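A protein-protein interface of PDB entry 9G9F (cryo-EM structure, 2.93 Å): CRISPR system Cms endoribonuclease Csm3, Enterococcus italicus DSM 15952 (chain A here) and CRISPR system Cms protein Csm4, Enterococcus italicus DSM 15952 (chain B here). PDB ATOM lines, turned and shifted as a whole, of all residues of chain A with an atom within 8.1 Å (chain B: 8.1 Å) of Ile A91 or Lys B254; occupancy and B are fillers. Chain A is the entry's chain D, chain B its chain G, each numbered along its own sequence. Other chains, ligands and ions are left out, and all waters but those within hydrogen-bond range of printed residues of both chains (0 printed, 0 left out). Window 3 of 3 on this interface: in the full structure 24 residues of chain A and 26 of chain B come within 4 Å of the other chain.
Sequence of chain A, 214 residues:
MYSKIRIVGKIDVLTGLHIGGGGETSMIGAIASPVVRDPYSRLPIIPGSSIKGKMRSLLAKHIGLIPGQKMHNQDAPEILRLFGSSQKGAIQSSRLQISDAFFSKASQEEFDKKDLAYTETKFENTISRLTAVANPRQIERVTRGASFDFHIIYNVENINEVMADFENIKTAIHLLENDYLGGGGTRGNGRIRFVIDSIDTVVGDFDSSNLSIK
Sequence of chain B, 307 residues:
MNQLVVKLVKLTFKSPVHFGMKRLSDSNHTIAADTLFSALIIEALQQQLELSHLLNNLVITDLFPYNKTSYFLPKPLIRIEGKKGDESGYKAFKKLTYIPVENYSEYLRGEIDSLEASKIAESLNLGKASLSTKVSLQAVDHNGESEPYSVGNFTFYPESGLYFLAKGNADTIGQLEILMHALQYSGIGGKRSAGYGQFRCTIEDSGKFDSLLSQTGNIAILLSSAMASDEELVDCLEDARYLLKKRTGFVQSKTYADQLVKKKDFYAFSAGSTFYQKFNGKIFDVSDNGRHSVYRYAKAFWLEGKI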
ATOM      1  N   TYR A   2      27.297  -0.549 -29.520  1.00  0.00           N
ATOM      2  CA  TYR A   2      27.455   0.147 -28.249  1.00  0.00           C
ATOM      3  C   TYR A   2      28.886   0.606 -28.066  1.00  0.00           C
ATOM      4  O   TYR A   2      29.821  -0.069 -28.495  1.00  0.00           O
ATOM      5  CB  TYR A   2      27.054  -0.752 -27.087  1.00  0.00           C
ATOM      6  CG  TYR A   2      26.543  -0.014 -25.876  1.00  0.00           C
ATOM      7  CD1 TYR A   2      25.210   0.346 -25.775  1.00  0.00           C
ATOM      8  CD2 TYR A   2      27.387   0.305 -24.827  1.00  0.00           C
ATOM      9  CE1 TYR A   2      24.732   1.009 -24.669  1.00  0.00           C
ATOM     10  CE2 TYR A   2      26.918   0.968 -23.715  1.00  0.00           C
ATOM     11  CZ  TYR A   2      25.588   1.317 -23.642  1.00  0.00           C
ATOM     12  OH  TYR A   2      25.108   1.978 -22.537  1.00  0.00           O
ATOM     13  N   LEU A  80      18.259  13.757 -17.396  1.00  0.00           N
ATOM     14  CA  LEU A  80      17.823  12.384 -17.164  1.00  0.00           C
ATOM     15  C   LEU A  80      18.574  11.400 -18.050  1.00  0.00           C
ATOM     16  O   LEU A  80      18.917  10.299 -17.611  1.00  0.00           O
ATOM     17  CB  LEU A  80      16.318  12.272 -17.390  1.00  0.00           C
ATOM     18  CG  LEU A  80      15.456  13.012 -16.368  1.00  0.00           C
ATOM     19  CD1 LEU A  80      14.064  12.423 -16.322  1.00  0.00           C
ATOM     20  CD2 LEU A  80      16.097  12.979 -14.992  1.00  0.00           C
ATOM     21  N   GLY A  84      20.732   9.197 -15.679  1.00  0.00           N
ATOM     22  CA  GLY A  84      19.784   8.154 -15.343  1.00  0.00           C
ATOM     23  C   GLY A  84      18.474   8.642 -14.768  1.00  0.00           C
ATOM     24  O   GLY A  84      18.427   9.658 -14.069  1.00  0.00           O
ATOM     25  N   SER A  85      17.397   7.918 -15.052  1.00  0.00           N
ATOM     26  CA  SER A  85      16.087   8.233 -14.510  1.00  0.00           C
ATOM     27  C   SER A  85      15.339   6.941 -14.238  1.00  0.00           C
ATOM     28  O   SER A  85      15.359   6.018 -15.058  1.00  0.00           O
ATOM     29  CB  SER A  85      15.277   9.113 -15.465  1.00  0.00           C
ATOM     30  OG  SER A  85      15.149   8.504 -16.736  1.00  0.00           O
ATOM     31  N   SER A  86      14.693   6.877 -13.078  1.00  0.00           N
ATOM     32  CA  SER A  86      13.845   5.755 -12.707  1.00  0.00           C
ATOM     33  C   SER A  86      12.365   6.097 -12.789  1.00  0.00           C
ATOM     34  O   SER A  86      11.531   5.307 -12.336  1.00  0.00           O
ATOM     35  CB  SER A  86      14.199   5.273 -11.301  1.00  0.00           C
ATOM     36  OG  SER A  86      13.318   5.821 -10.339  1.00  0.00           O
ATOM     37  N   GLN A  87      12.022   7.245 -13.368  1.00  0.00           N
ATOM     38  CA  GLN A  87      10.645   7.712 -13.390  1.00  0.00           C
ATOM     39  C   GLN A  87       9.766   6.777 -14.211  1.00  0.00           C
ATOM     40  O   GLN A  87      10.237   6.021 -15.064  1.00  0.00           O
ATOM     41  CB  GLN A  87      10.566   9.129 -13.955  1.00  0.00           C
ATOM     42  CG  GLN A  87      11.210  10.185 -13.077  1.00  0.00           C
ATOM     43  CD  GLN A  87      11.048  11.584 -13.638  1.00  0.00           C
ATOM     44  OE1 GLN A  87      10.355  11.789 -14.635  1.00  0.00           O
ATOM     45  NE2 GLN A  87      11.688  12.555 -12.999  1.00  0.00           N
ATOM     46  N   LYS A  88       8.466   6.835 -13.930  1.00  0.00           N
ATOM     47  CA  LYS A  88       7.510   5.951 -14.584  1.00  0.00           C
ATOM     48  C   LYS A  88       7.482   6.212 -16.084  1.00  0.00           C
ATOM     49  O   LYS A  88       7.404   7.360 -16.526  1.00  0.00           O
ATOM     50  CB  LYS A  88       6.110   6.144 -13.994  1.00  0.00           C
ATOM     51  CG  LYS A  88       6.048   6.601 -12.536  1.00  0.00           C
ATOM     52  CD  LYS A  88       6.864   5.727 -11.592  1.00  0.00           C
ATOM     53  CE  LYS A  88       6.746   6.218 -10.161  1.00  0.00           C
ATOM     54  NZ  LYS A  88       5.347   6.132  -9.659  1.00  0.00           N
ATOM     55  N   GLY A  89       7.539   5.140 -16.865  1.00  0.00           N
ATOM     56  CA  GLY A  89       7.529   5.261 -18.307  1.00  0.00           C
ATOM     57  C   GLY A  89       8.897   5.546 -18.885  1.00  0.00           C
ATOM     58  O   GLY A  89       9.411   4.771 -19.695  1.00  0.00           O
ATOM     59  N   ALA A  90       9.500   6.659 -18.472  1.00  0.00           N
ATOM     60  CA  ALA A  90      10.819   7.057 -18.962  1.00  0.00           C
ATOM     61  C   ALA A  90      11.878   6.425 -18.070  1.00  0.00           C
ATOM     62  O   ALA A  90      12.329   7.014 -17.088  1.00  0.00           O
ATOM     63  CB  ALA A  90      10.946   8.575 -18.993  1.00  0.00           C
ATOM     64  N   ILE A  91      12.276   5.207 -18.417  1.00  0.00           N
ATOM     65  CA  ILE A  91      13.361   4.505 -17.741  1.00  0.00           C
ATOM     66  C   ILE A  91      14.581   4.607 -18.644  1.00  0.00           C
ATOM     67  O   ILE A  91      14.593   4.057 -19.749  1.00  0.00           O
ATOM     68  CB  ILE A  91      13.002   3.041 -17.451  1.00  0.00           C
ATOM     69  CG1 ILE A  91      11.935   2.947 -16.358  1.00  0.00           C
ATOM     70  CG2 ILE A  91      14.240   2.262 -17.043  1.00  0.00           C
ATOM     71  CD1 ILE A  91      12.443   3.263 -14.977  1.00  0.00           C
ATOM     72  N   GLN A  92      15.608   5.313 -18.181  1.00  0.00           N
ATOM     73  CA  GLN A  92      16.817   5.533 -18.960  1.00  0.00           C
ATOM     74  C   GLN A  92      18.029   5.125 -18.142  1.00  0.00           C
ATOM     75  O   GLN A  92      18.138   5.485 -16.965  1.00  0.00           O
ATOM     76  CB  GLN A  92      16.944   6.996 -19.390  1.00  0.00           C
ATOM     77  CG  GLN A  92      16.265   7.321 -20.704  1.00  0.00           C
ATOM     78  CD  GLN A  92      16.028   8.804 -20.875  1.00  0.00           C
ATOM     79  OE1 GLN A  92      15.722   9.507 -19.912  1.00  0.00           O
ATOM     80  NE2 GLN A  92      16.170   9.290 -22.101  1.00  0.00           N
ATOM     81  N   SER A  93      18.931   4.373 -18.764  1.00  0.00           N
ATOM     82  CA  SER A  93      20.181   4.019 -18.112  1.00  0.00           C
ATOM     83  C   SER A  93      21.110   5.224 -18.097  1.00  0.00           C
ATOM     84  O   SER A  93      21.275   5.904 -19.114  1.00  0.00           O
ATOM     85  CB  SER A  93      20.842   2.847 -18.834  1.00  0.00           C
ATOM     86  OG  SER A  93      19.948   1.757 -18.953  1.00  0.00           O
ATOM     87  N   SER A  94      21.708   5.496 -16.941  1.00  0.00           N
ATOM     88  CA  SER A  94      22.632   6.613 -16.830  1.00  0.00           C
ATOM     89  C   SER A  94      23.843   6.386 -17.723  1.00  0.00           C
ATOM     90  O   SER A  94      24.399   5.288 -17.776  1.00  0.00           O
ATOM     91  CB  SER A  94      23.075   6.797 -15.381  1.00  0.00           C
ATOM     92  OG  SER A  94      23.980   7.875 -15.264  1.00  0.00           O
ATOM     93  N   GLU A 157      24.748   5.371 -25.858  1.00  0.00           N
ATOM     94  CA  GLU A 157      23.528   4.652 -26.193  1.00  0.00           C
ATOM     95  C   GLU A 157      23.089   4.964 -27.617  1.00  0.00           C
ATOM     96  O   GLU A 157      22.629   4.071 -28.339  1.00  0.00           O
ATOM     97  CB  GLU A 157      22.424   5.001 -25.200  1.00  0.00           C
ATOM     98  CG  GLU A 157      22.844   4.880 -23.751  1.00  0.00           C
ATOM     99  CD  GLU A 157      21.662   4.843 -22.810  1.00  0.00           C
ATOM    100  OE1 GLU A 157      20.516   4.964 -23.290  1.00  0.00           O
ATOM    101  OE2 GLU A 157      21.878   4.689 -21.591  1.00  0.00           O
ATOM    102  N   GLN B  46      23.422  -5.161 -24.569  1.00  0.00           N
ATOM    103  CA  GLN B  46      23.943  -3.844 -24.918  1.00  0.00           C
ATOM    104  C   GLN B  46      24.902  -3.924 -26.099  1.00  0.00           C
ATOM    105  O   GLN B  46      24.838  -3.100 -27.017  1.00  0.00           O
ATOM    106  CB  GLN B  46      24.627  -3.209 -23.710  1.00  0.00           C
ATOM    107  CG  GLN B  46      23.660  -2.702 -22.662  1.00  0.00           C
ATOM    108  CD  GLN B  46      24.359  -2.069 -21.477  1.00  0.00           C
ATOM    109  OE1 GLN B  46      25.563  -1.826 -21.509  1.00  0.00           O
ATOM    110  NE2 GLN B  46      23.604  -1.799 -20.421  1.00  0.00           N
ATOM    111  N   VAL B 251      13.661  -6.035 -11.227  1.00  0.00           N
ATOM    112  CA  VAL B 251      14.146  -6.208 -12.592  1.00  0.00           C
ATOM    113  C   VAL B 251      14.877  -4.951 -13.035  1.00  0.00           C
ATOM    114  O   VAL B 251      14.379  -3.831 -12.869  1.00  0.00           O
ATOM    115  CB  VAL B 251      12.984  -6.542 -13.542  1.00  0.00           C
ATOM    116  CG1 VAL B 251      13.432  -6.444 -14.984  1.00  0.00           C
ATOM    117  CG2 VAL B 251      12.456  -7.927 -13.259  1.00  0.00           C
ATOM    118  N   GLN B 252      16.067  -5.130 -13.601  1.00  0.00           N
ATOM    119  CA  GLN B 252      16.890  -4.032 -14.105  1.00  0.00           C
ATOM    120  C   GLN B 252      16.862  -4.076 -15.629  1.00  0.00           C
ATOM    121  O   GLN B 252      17.609  -4.835 -16.252  1.00  0.00           O
ATOM    122  CB  GLN B 252      18.316  -4.132 -13.576  1.00  0.00           C
ATOM    123  CG  GLN B 252      19.263  -3.104 -14.154  1.00  0.00           C
ATOM    124  CD  GLN B 252      20.678  -3.286 -13.663  1.00  0.00           C
ATOM    125  OE1 GLN B 252      21.585  -3.554 -14.446  1.00  0.00           O
ATOM    126  NE2 GLN B 252      20.877  -3.138 -12.364  1.00  0.00           N
ATOM    127  N   SER B 253      15.996  -3.262 -16.223  1.00  0.00           N
ATOM    128  CA  SER B 253      15.895  -3.156 -17.672  1.00  0.00           C
ATOM    129  C   SER B 253      15.061  -1.927 -17.997  1.00  0.00           C
ATOM    130  O   SER B 253      14.455  -1.313 -17.117  1.00  0.00           O
ATOM    131  CB  SER B 253      15.281  -4.408 -18.296  1.00  0.00           C
ATOM    132  OG  SER B 253      13.976  -4.628 -17.802  1.00  0.00           O
ATOM    133  N   LYS B 254      15.045  -1.575 -19.282  1.00  0.00           N
ATOM    134  CA  LYS B 254      14.254  -0.456 -19.768  1.00  0.00           C
ATOM    135  C   LYS B 254      13.002  -0.889 -20.515  1.00  0.00           C
ATOM    136  O   LYS B 254      12.050  -0.106 -20.601  1.00  0.00           O
ATOM    137  CB  LYS B 254      15.099   0.426 -20.695  1.00  0.00           C
ATOM    138  CG  LYS B 254      16.176   1.234 -19.993  1.00  0.00           C
ATOM    139  CD  LYS B 254      17.305   1.596 -20.947  1.00  0.00           C
ATOM    140  CE  LYS B 254      16.791   1.959 -22.333  1.00  0.00           C
ATOM    141  NZ  LYS B 254      15.938   3.175 -22.322  1.00  0.00           N
ATOM    142  N   THR B 255      12.978  -2.107 -21.045  1.00  0.00           N
ATOM    143  CA  THR B 255      11.898  -2.588 -21.898  1.00  0.00           C
ATOM    144  C   THR B 255      11.061  -3.662 -21.210  1.00  0.00           C
ATOM    145  O   THR B 255      10.567  -4.589 -21.851  1.00  0.00           O
ATOM    146  CB  THR B 255      12.458  -3.114 -23.215  1.00  0.00           C
ATOM    147  OG1 THR B 255      12.982  -4.433 -23.025  1.00  0.00           O
ATOM    148  CG2 THR B 255      13.570  -2.209 -23.708  1.00  0.00           C
ATOM    149  N   TYR B 256      10.872  -3.540 -19.898  1.00  0.00           N
ATOM    150  CA  TYR B 256      10.088  -4.503 -19.135  1.00  0.00           C
ATOM    151  C   TYR B 256       8.738  -3.954 -18.705  1.00  0.00           C
ATOM    152  O   TYR B 256       7.709  -4.590 -18.944  1.00  0.00           O
ATOM    153  CB  TYR B 256      10.872  -4.966 -17.901  1.00  0.00           C
ATOM    154  CG  TYR B 256      10.290  -6.184 -17.220  1.00  0.00           C
ATOM    155  CD1 TYR B 256      10.449  -7.450 -17.764  1.00  0.00           C
ATOM    156  CD2 TYR B 256       9.586  -6.066 -16.032  1.00  0.00           C
ATOM    157  CE1 TYR B 256       9.919  -8.559 -17.147  1.00  0.00           C
ATOM    158  CE2 TYR B 256       9.055  -7.170 -15.410  1.00  0.00           C
ATOM    159  CZ  TYR B 256       9.225  -8.411 -15.971  1.00  0.00           C
ATOM    160  OH  TYR B 256       8.697  -9.514 -15.348  1.00  0.00           O
ATOM    161  N   ALA B 257       8.714  -2.788 -18.070  1.00  0.00           N
ATOM    162  CA  ALA B 257       7.465  -2.196 -17.619  1.00  0.00           C
ATOM    163  C   ALA B 257       7.665  -0.698 -17.455  1.00  0.00           C
ATOM    164  O   ALA B 257       8.792  -0.197 -17.459  1.00  0.00           O
ATOM    165  CB  ALA B 257       6.982  -2.834 -16.313  1.00  0.00           C
ATOM    166  N   ASP B 258       6.547   0.015 -17.318  1.00  0.00           N
ATOM    167  CA  ASP B 258       6.611   1.451 -17.070  1.00  0.00           C
ATOM    168  C   ASP B 258       7.299   1.746 -15.743  1.00  0.00           C
ATOM    169  O   ASP B 258       8.117   2.667 -15.651  1.00  0.00           O
ATOM    170  CB  ASP B 258       5.206   2.053 -17.092  1.00  0.00           C
ATOM    171  CG  ASP B 258       4.481   1.796 -18.400  1.00  0.00           C
ATOM    172  OD1 ASP B 258       4.118   0.632 -18.666  1.00  0.00           O
ATOM    173  OD2 ASP B 258       4.275   2.762 -19.164  1.00  0.00           O
ATOM    174  N   GLN B 259       6.984   0.974 -14.708  1.00  0.00           N
ATOM    175  CA  GLN B 259       7.642   1.083 -13.417  1.00  0.00           C
ATOM    176  C   GLN B 259       8.363  -0.221 -13.102  1.00  0.00           C
ATOM    177  O   GLN B 259       8.024  -1.284 -13.628  1.00  0.00           O
ATOM    178  CB  GLN B 259       6.641   1.417 -12.307  1.00  0.00           C
ATOM    179  CG  GLN B 259       5.528   0.399 -12.149  1.00  0.00           C
ATOM    180  CD  GLN B 259       4.690   0.647 -10.912  1.00  0.00           C
ATOM    181  OE1 GLN B 259       4.935   1.591 -10.161  1.00  0.00           O
ATOM    182  NE2 GLN B 259       3.695  -0.204 -10.691  1.00  0.00           N
ATOM    183  N   LEU B 260       9.372  -0.124 -12.238  1.00  0.00           N
ATOM    184  CA  LEU B 260      10.191  -1.281 -11.903  1.00  0.00           C
ATOM    185  C   LEU B 260       9.354  -2.354 -11.217  1.00  0.00           C
ATOM    186  O   LEU B 260       8.576  -2.066 -10.304  1.00  0.00           O
ATOM    187  CB  LEU B 260      11.353  -0.855 -11.009  1.00  0.00           C
ATOM    188  CG  LEU B 260      12.362   0.095 -11.654  1.00  0.00           C
ATOM    189  CD1 LEU B 260      13.026   0.950 -10.599  1.00  0.00           C
ATOM    190  CD2 LEU B 260      13.399  -0.677 -12.447  1.00  0.00           C
ATOM    191  N   ARG B 291       7.640  -7.619 -20.947  1.00  0.00           N
ATOM    192  CA  ARG B 291       7.855  -7.721 -22.383  1.00  0.00           C
ATOM    193  C   ARG B 291       9.000  -8.655 -22.754  1.00  0.00           C
ATOM    194  O   ARG B 291       9.198  -8.922 -23.943  1.00  0.00           O
ATOM    195  CB  ARG B 291       8.110  -6.332 -22.969  1.00  0.00           C
ATOM    196  CG  ARG B 291       6.876  -5.450 -23.009  1.00  0.00           C
ATOM    197  CD  ARG B 291       7.180  -4.087 -23.601  1.00  0.00           C
ATOM    198  NE  ARG B 291       7.574  -3.122 -22.583  1.00  0.00           N
ATOM    199  CZ  ARG B 291       6.721  -2.411 -21.859  1.00  0.00           C
ATOM    200  NH1 ARG B 291       5.413  -2.546 -22.002  1.00  0.00           N
ATOM    201  NH2 ARG B 291       7.191  -1.541 -20.970  1.00  0.00           N
ATOM    202  N   HIS B 292       9.753  -9.151 -21.775  1.00  0.00           N
ATOM    203  CA  HIS B 292      10.887 -10.021 -22.037  1.00  0.00           C
ATOM    204  C   HIS B 292      11.142 -10.882 -20.811  1.00  0.00           C
ATOM    205  O   HIS B 292      10.999 -10.423 -19.675  1.00  0.00           O
ATOM    206  CB  HIS B 292      12.136  -9.210 -22.387  1.00  0.00           C
ATOM    207  CG  HIS B 292      12.560  -8.270 -21.303  1.00  0.00           C
ATOM    208  ND1 HIS B 292      13.396  -8.647 -20.277  1.00  0.00           N
ATOM    209  CD2 HIS B 292      12.246  -6.974 -21.076  1.00  0.00           C
ATOM    210  CE1 HIS B 292      13.588  -7.619 -19.470  1.00  0.00           C
ATOM    211  NE2 HIS B 292      12.900  -6.591 -19.932  1.00  0.00           N
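O of Ile A91 is in hydrogen-bond range of NZ of Lys B254 (3.0 Å).
O of Asp B258 lies within hydrogen-bond range of N of Gly A89 (2.8 Å).
OG of Ser B253 lies within hydrogen-bond range of NE2 of His B292, 3.1 Å away.
Printed residues of chain B that touch a printed residue of chain A: Gln B46, Ser B253, Lys B254 and Asp B258.
Hydrophobic or aromatic side chains of chain A that line the printed part of chain B: Tyr A2 and Ile A91.
Among the printed residues, 7 pairs touch across the chains.
Among the printed residues, no Asp or Glu carboxylate lies within 4 Å of a Lys or Arg side-chain nitrogen of the other chain.
Among the printed residues, merely in contact across the chains: Tyr A2 with Gln B46 (3.2 Å), Lys A88 with Asp B258 (3.5 Å), Ile A91 with Ser B253 (3.6 Å), Ile A91 with Asp B258 (3.9 Å) and Ser A93 with Lys B254 (3.3 Å).
Printed residues of chain B within 4 Å of Tyr A2: Gln B46 (3.2 Å).
Of the printed residues of chain B, Lys A88 touches Asp B258 (3.5 Å).
Printed residues of chain B within 4 Å of Gly A89: Asp B258.
No residue of chain B comes within 4 Å of Ala A90.
Printed residues of chain B within 4 Å of Ile A91: Ser B253, Lys B254 and Asp B258.
Of the printed residues of chain B, Ser A93 touches Lys B254 (3.3 Å).
Printed residues of chain A within 4 Å of Gln B46: Tyr A2.
Of the printed residues of chain A, Ser B253 touches Ile A91 (3.6 Å).
Of chain A, only Ile A91 and Ser A93 come within 4 Å of Lys B254.
Leu B260 touches none of the printed residues of chain A.
The nearest printed residue of chain B that does not touch Ile A91 is Ala B257 (4.6 Å).
The nearest printed residue of chain B that does not touch Tyr A2 is Lys B254 (8.0 Å).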
